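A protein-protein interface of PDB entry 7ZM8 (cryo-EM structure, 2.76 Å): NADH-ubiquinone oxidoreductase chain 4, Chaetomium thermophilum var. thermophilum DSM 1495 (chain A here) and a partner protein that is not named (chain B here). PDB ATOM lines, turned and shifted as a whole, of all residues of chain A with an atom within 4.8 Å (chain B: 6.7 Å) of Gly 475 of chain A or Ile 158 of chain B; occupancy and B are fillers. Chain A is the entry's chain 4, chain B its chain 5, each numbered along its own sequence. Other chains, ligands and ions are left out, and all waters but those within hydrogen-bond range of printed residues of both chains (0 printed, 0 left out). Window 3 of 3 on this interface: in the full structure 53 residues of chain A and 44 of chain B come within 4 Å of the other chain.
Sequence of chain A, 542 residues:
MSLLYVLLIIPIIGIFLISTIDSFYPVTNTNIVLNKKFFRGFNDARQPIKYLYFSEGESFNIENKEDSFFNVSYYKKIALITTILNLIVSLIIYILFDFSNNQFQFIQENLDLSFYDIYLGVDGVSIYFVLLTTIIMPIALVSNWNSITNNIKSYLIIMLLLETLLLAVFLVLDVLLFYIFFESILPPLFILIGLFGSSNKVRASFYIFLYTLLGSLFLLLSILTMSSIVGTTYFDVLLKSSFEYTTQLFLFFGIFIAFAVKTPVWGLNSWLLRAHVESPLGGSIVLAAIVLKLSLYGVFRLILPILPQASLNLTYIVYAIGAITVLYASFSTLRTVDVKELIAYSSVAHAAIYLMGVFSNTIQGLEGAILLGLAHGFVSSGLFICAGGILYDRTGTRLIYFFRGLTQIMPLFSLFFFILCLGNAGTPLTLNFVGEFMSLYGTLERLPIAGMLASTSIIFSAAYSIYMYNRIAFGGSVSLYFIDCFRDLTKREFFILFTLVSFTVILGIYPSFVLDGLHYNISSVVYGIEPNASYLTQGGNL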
ATOM      1  N   ARG A 404       2.888   5.618  33.293  1.00  0.00           N
ATOM      2  CA  ARG A 404       2.569   6.560  32.199  1.00  0.00           C
ATOM      3  C   ARG A 404       2.049   5.770  31.001  1.00  0.00           C
ATOM      4  O   ARG A 404       2.512   4.641  30.819  1.00  0.00           O
ATOM      5  CB  ARG A 404       3.814   7.367  31.826  1.00  0.00           C
ATOM      6  CG  ARG A 404       3.612   8.462  30.796  1.00  0.00           C
ATOM      7  CD  ARG A 404       4.975   9.041  30.490  1.00  0.00           C
ATOM      8  NE  ARG A 404       5.862   8.056  29.893  1.00  0.00           N
ATOM      9  CZ  ARG A 404       7.136   8.275  29.605  1.00  0.00           C
ATOM     10  NH1 ARG A 404       7.678   9.445  29.873  1.00  0.00           N
ATOM     11  NH2 ARG A 404       7.868   7.324  29.056  1.00  0.00           N
ATOM     12  N   ASN A 470      -4.925  11.281  33.647  1.00  0.00           N
ATOM     13  CA  ASN A 470      -3.987  11.652  32.596  1.00  0.00           C
ATOM     14  C   ASN A 470      -2.552  11.272  32.912  1.00  0.00           C
ATOM     15  O   ASN A 470      -1.717  11.275  32.008  1.00  0.00           O
ATOM     16  CB  ASN A 470      -4.050  13.153  32.321  1.00  0.00           C
ATOM     17  CG  ASN A 470      -5.226  13.542  31.472  1.00  0.00           C
ATOM     18  OD1 ASN A 470      -5.527  12.892  30.481  1.00  0.00           O
ATOM     19  ND2 ASN A 470      -5.903  14.603  31.856  1.00  0.00           N
ATOM     20  N   ALA A 473      -3.090   6.580  32.772  1.00  0.00           N
ATOM     21  CA  ALA A 473      -3.586   6.026  31.517  1.00  0.00           C
ATOM     22  C   ALA A 473      -2.991   6.747  30.321  1.00  0.00           C
ATOM     23  O   ALA A 473      -2.607   6.115  29.335  1.00  0.00           O
ATOM     24  CB  ALA A 473      -5.107   6.102  31.477  1.00  0.00           C
ATOM     25  N   PHE A 474      -2.872   8.057  30.409  1.00  0.00           N
ATOM     26  CA  PHE A 474      -2.412   8.948  29.361  1.00  0.00           C
ATOM     27  C   PHE A 474      -1.091   9.543  29.822  1.00  0.00           C
ATOM     28  O   PHE A 474      -0.461   9.053  30.763  1.00  0.00           O
ATOM     29  CB  PHE A 474      -3.442  10.048  29.077  1.00  0.00           C
ATOM     30  CG  PHE A 474      -4.725   9.568  28.465  1.00  0.00           C
ATOM     31  CD1 PHE A 474      -4.850   8.288  27.964  1.00  0.00           C
ATOM     32  CD2 PHE A 474      -5.813  10.416  28.384  1.00  0.00           C
ATOM     33  CE1 PHE A 474      -6.034   7.860  27.408  1.00  0.00           C
ATOM     34  CE2 PHE A 474      -6.998   9.992  27.822  1.00  0.00           C
ATOM     35  CZ  PHE A 474      -7.105   8.712  27.334  1.00  0.00           C
ATOM     36  N   GLY A 475      -0.707  10.676  29.266  1.00  0.00           N
ATOM     37  CA  GLY A 475       0.475  11.373  29.808  1.00  0.00           C
ATOM     38  C   GLY A 475       1.721  11.084  29.032  1.00  0.00           C
ATOM     39  O   GLY A 475       2.801  11.466  29.479  1.00  0.00           O
ATOM     40  N   GLY A 476       1.559  10.442  27.889  1.00  0.00           N
ATOM     41  CA  GLY A 476       2.728  10.060  27.108  1.00  0.00           C
ATOM     42  C   GLY A 476       2.632   8.619  26.731  1.00  0.00           C
ATOM     43  O   GLY A 476       1.558   8.057  26.870  1.00  0.00           O
ATOM     44  N   SER A 477       3.721   8.058  26.245  1.00  0.00           N
ATOM     45  CA  SER A 477       3.765   6.643  25.845  1.00  0.00           C
ATOM     46  C   SER A 477       4.005   5.773  27.067  1.00  0.00           C
ATOM     47  O   SER A 477       4.385   6.303  28.098  1.00  0.00           O
ATOM     48  CB  SER A 477       4.808   6.451  24.806  1.00  0.00           C
ATOM     49  OG  SER A 477       4.662   7.414  23.786  1.00  0.00           O
ATOM     50  N   TRP B 154      -4.929  11.944  20.706  1.00  0.00           N
ATOM     51  CA  TRP B 154      -3.526  11.457  20.640  1.00  0.00           C
ATOM     52  C   TRP B 154      -2.928  11.601  22.040  1.00  0.00           C
ATOM     53  O   TRP B 154      -2.264  12.619  22.289  1.00  0.00           O
ATOM     54  CB  TRP B 154      -2.737  12.228  19.580  1.00  0.00           C
ATOM     55  CG  TRP B 154      -3.263  12.057  18.190  1.00  0.00           C
ATOM     56  CD1 TRP B 154      -3.474  10.881  17.531  1.00  0.00           C
ATOM     57  CD2 TRP B 154      -3.628  13.101  17.271  1.00  0.00           C
ATOM     58  NE1 TRP B 154      -3.953  11.122  16.271  1.00  0.00           N
ATOM     59  CE2 TRP B 154      -4.058  12.473  16.082  1.00  0.00           C
ATOM     60  CE3 TRP B 154      -3.635  14.498  17.334  1.00  0.00           C
ATOM     61  CZ2 TRP B 154      -4.487  13.197  14.973  1.00  0.00           C
ATOM     62  CZ3 TRP B 154      -4.062  15.213  16.238  1.00  0.00           C
ATOM     63  CH2 TRP B 154      -4.476  14.568  15.073  1.00  0.00           C
ATOM     64  N   PHE B 155      -3.161  10.619  22.915  1.00  0.00           N
ATOM     65  CA  PHE B 155      -2.720  10.690  24.336  1.00  0.00           C
ATOM     66  C   PHE B 155      -1.193  10.685  24.481  1.00  0.00           C
ATOM     67  O   PHE B 155      -0.695  11.117  25.529  1.00  0.00           O
ATOM     68  CB  PHE B 155      -3.399   9.590  25.150  1.00  0.00           C
ATOM     69  CG  PHE B 155      -3.593   8.286  24.422  1.00  0.00           C
ATOM     70  CD1 PHE B 155      -2.536   7.408  24.242  1.00  0.00           C
ATOM     71  CD2 PHE B 155      -4.837   7.931  23.927  1.00  0.00           C
ATOM     72  CE1 PHE B 155      -2.718   6.209  23.573  1.00  0.00           C
ATOM     73  CE2 PHE B 155      -5.017   6.730  23.261  1.00  0.00           C
ATOM     74  CZ  PHE B 155      -3.955   5.875  23.083  1.00  0.00           C
ATOM     75  N   THR B 156      -0.480  10.170  23.483  1.00  0.00           N
ATOM     76  CA  THR B 156       1.004  10.102  23.534  1.00  0.00           C
ATOM     77  C   THR B 156       1.590  11.517  23.628  1.00  0.00           C
ATOM     78  O   THR B 156       2.628  11.668  24.281  1.00  0.00           O
ATOM     79  CB  THR B 156       1.560   9.209  22.420  1.00  0.00           C
ATOM     80  OG1 THR B 156       1.028   9.666  21.178  1.00  0.00           O
ATOM     81  CG2 THR B 156       1.200   7.754  22.613  1.00  0.00           C
ATOM     82  N   ARG B 157       0.975  12.502  22.968  1.00  0.00           N
ATOM     83  CA  ARG B 157       1.508  13.889  22.979  1.00  0.00           C
ATOM     84  C   ARG B 157       1.151  14.581  24.301  1.00  0.00           C
ATOM     85  O   ARG B 157      -0.046  14.660  24.621  1.00  0.00           O
ATOM     86  CB  ARG B 157       0.987  14.634  21.749  1.00  0.00           C
ATOM     87  CG  ARG B 157       1.307  16.118  21.706  1.00  0.00           C
ATOM     88  CD  ARG B 157       0.897  16.633  20.342  1.00  0.00           C
ATOM     89  NE  ARG B 157       0.865  18.083  20.246  1.00  0.00           N
ATOM     90  CZ  ARG B 157       1.917  18.835  19.957  1.00  0.00           C
ATOM     91  NH1 ARG B 157       1.793  20.148  19.886  1.00  0.00           N
ATOM     92  NH2 ARG B 157       3.092  18.268  19.753  1.00  0.00           N
ATOM     93  N   ILE B 158       2.159  15.059  25.039  1.00  0.00           N
ATOM     94  CA  ILE B 158       1.945  15.741  26.352  1.00  0.00           C
ATOM     95  C   ILE B 158       1.195  17.065  26.161  1.00  0.00           C
ATOM     96  O   ILE B 158       0.326  17.367  26.989  1.00  0.00           O
ATOM     97  CB  ILE B 158       3.281  15.903  27.107  1.00  0.00           C
ATOM     98  CG1 ILE B 158       3.873  14.541  27.475  1.00  0.00           C
ATOM     99  CG2 ILE B 158       3.117  16.783  28.336  1.00  0.00           C
ATOM    100  CD1 ILE B 158       5.026  14.613  28.444  1.00  0.00           C
ATOM    101  N   ALA B 159       1.522  17.822  25.111  1.00  0.00           N
ATOM    102  CA  ALA B 159       0.830  19.103  24.839  1.00  0.00           C
ATOM    103  C   ALA B 159      -0.678  18.859  24.805  1.00  0.00           C
ATOM    104  O   ALA B 159      -1.413  19.662  25.398  1.00  0.00           O
ATOM    105  CB  ALA B 159       1.319  19.669  23.536  1.00  0.00           C
ATOM    106  N   ALA B 160      -1.109  17.794  24.132  1.00  0.00           N
ATOM    107  CA  ALA B 160      -2.535  17.433  24.020  1.00  0.00           C
ATOM    108  C   ALA B 160      -3.123  17.157  25.410  1.00  0.00           C
ATOM    109  O   ALA B 160      -4.290  17.497  25.620  1.00  0.00           O
ATOM    110  CB  ALA B 160      -2.607  16.218  23.137  1.00  0.00           C
ATOM    111  N   ASN B 161      -2.329  16.581  26.316  1.00  0.00           N
ATOM    112  CA  ASN B 161      -2.811  16.180  27.658  1.00  0.00           C
ATOM    113  C   ASN B 161      -2.909  17.429  28.519  1.00  0.00           C
ATOM    114  O   ASN B 161      -3.762  17.440  29.400  1.00  0.00           O
ATOM    115  CB  ASN B 161      -1.798  15.245  28.318  1.00  0.00           C
ATOM    116  CG  ASN B 161      -1.987  13.782  28.001  1.00  0.00           C
ATOM    117  OD1 ASN B 161      -2.686  13.080  28.722  1.00  0.00           O
ATOM    118  ND2 ASN B 161      -1.336  13.308  26.956  1.00  0.00           N
ATOM    119  N   GLN B 162      -2.044  18.421  28.304  1.00  0.00           N
ATOM    120  CA  GLN B 162      -2.213  19.697  28.989  1.00  0.00           C
ATOM    121  C   GLN B 162      -3.444  20.439  28.490  1.00  0.00           C
ATOM    122  O   GLN B 162      -4.194  21.011  29.285  1.00  0.00           O
ATOM    123  CB  GLN B 162      -0.965  20.554  28.805  1.00  0.00           C
ATOM    124  CG  GLN B 162       0.325  19.834  29.081  1.00  0.00           C
ATOM    125  CD  GLN B 162       1.349  20.723  29.721  1.00  0.00           C
ATOM    126  OE1 GLN B 162       1.794  21.701  29.128  1.00  0.00           O
ATOM    127  NE2 GLN B 162       1.725  20.400  30.946  1.00  0.00           N
ATOM    128  N   SER B 163      -3.658  20.456  27.177  1.00  0.00           N
ATOM    129  CA  SER B 163      -4.768  21.213  26.613  1.00  0.00           C
ATOM    130  C   SER B 163      -6.113  20.597  26.965  1.00  0.00           C
ATOM    131  O   SER B 163      -7.115  21.314  27.049  1.00  0.00           O
ATOM    132  CB  SER B 163      -4.611  21.307  25.100  1.00  0.00           C
ATOM    133  OG  SER B 163      -3.356  21.860  24.762  1.00  0.00           O
ATOM    134  N   GLU B 238      -5.469  21.433  19.678  1.00  0.00           N
ATOM    135  CA  GLU B 238      -4.534  20.285  19.717  1.00  0.00           C
ATOM    136  C   GLU B 238      -5.186  19.031  19.119  1.00  0.00           C
ATOM    137  O   GLU B 238      -4.464  18.212  18.551  1.00  0.00           O
ATOM    138  CB  GLU B 238      -4.073  20.086  21.155  1.00  0.00           C
ATOM    139  CG  GLU B 238      -3.102  21.152  21.614  1.00  0.00           C
ATOM    140  CD  GLU B 238      -1.652  20.802  21.352  1.00  0.00           C
ATOM    141  OE1 GLU B 238      -1.388  19.634  21.028  1.00  0.00           O
ATOM    142  OE2 GLU B 238      -0.795  21.699  21.470  1.00  0.00           O
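Phe 474 of chain A touches Phe 155 of chain B (CD1 to CB, 3.4 Å).
CB of Phe 474 of chain A touches OD1 of Asn 161 of chain B (3.1 Å).
Gly 475 of chain A touches Phe 155 of chain B.
CG1 of Ile 158 of chain B touches O of Gly 475 of chain A, 3.8 Å away.
Gly 476 of chain A touches Thr 156 of chain B (CA to O, 3.3 Å).
Ser 477 of chain A touches Thr 156 of chain B (OG to CG2, 3.7 Å).
Of the 11 printed residues of chain B, 4 touch a printed residue of chain A.
Printed residues of chain B that touch a printed residue of chain A: Phe 155, Thr 156, Ile 158 and Asn 161.
Hydrophobic or aromatic side chains of chain B that line the printed part of chain A: Phe 155 and Ile 158.
Hydrophobic or aromatic side chains of chain A that line the printed part of chain B: Phe 474.
Of the printed residues of chain B, Asn 470 of chain A touches Asn 161.
Printed residues of chain B within 4 Å of Phe 474 of chain A: Phe 155 and Asn 161.
Of chain B, only Phe 155, Ile 158 and Asn 161 come within 4 Å of Gly 475 of chain A.
Of the printed residues of chain B, Ser 477 of chain A touches Thr 156 (3.7 Å).
Of the printed residues of chain A, Phe 155 of chain B touches Phe 474, Gly 475 and Gly 476.
Of the printed residues of chain A, Thr 156 of chain B touches Gly 476 and Ser 477.
Ile 158 of chain B touches just one residue of chain A: Gly 475 (3.8 Å).
Glu 238 of chain B touches none of the printed residues of chain A.
The nearest residue of chain A that does not touch Ile 158 of chain B is Gly 476 of chain A (4.6 Å).
OD1 of Asn 470 of chain A sits close to OD1 of Asn 161 of chain B, 3.3 Å away.
The backbone NH of Gly 476 of chain A lies within hydrogen-bond range of the backbone carbonyl oxygen of Phe 155 of chain B (3.3 Å).
N of Gly 475 of chain A sits at hydrogen-bond distance from OD1 of Asn 161 of chain B, at 3.2 Å.
The backbone carbonyl oxygen (O) of Phe 155 of chain B lies within hydrogen-bond range of the side-chain amide nitrogen (ND2) of Asn 161 of chain B (2.7 Å).
NE of Arg 404 of chain A sits at hydrogen-bond distance from O of Ser 477 of chain A (2.9 Å).
O of Arg 157 of chain B sits at hydrogen-bond distance from ND2 of Asn 161 of chain B (3.0 Å).
The backbone NH (N) of Gly 475 of chain A sits at hydrogen-bond distance from the backbone carbonyl oxygen (O) of Asn 470 of chain A.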
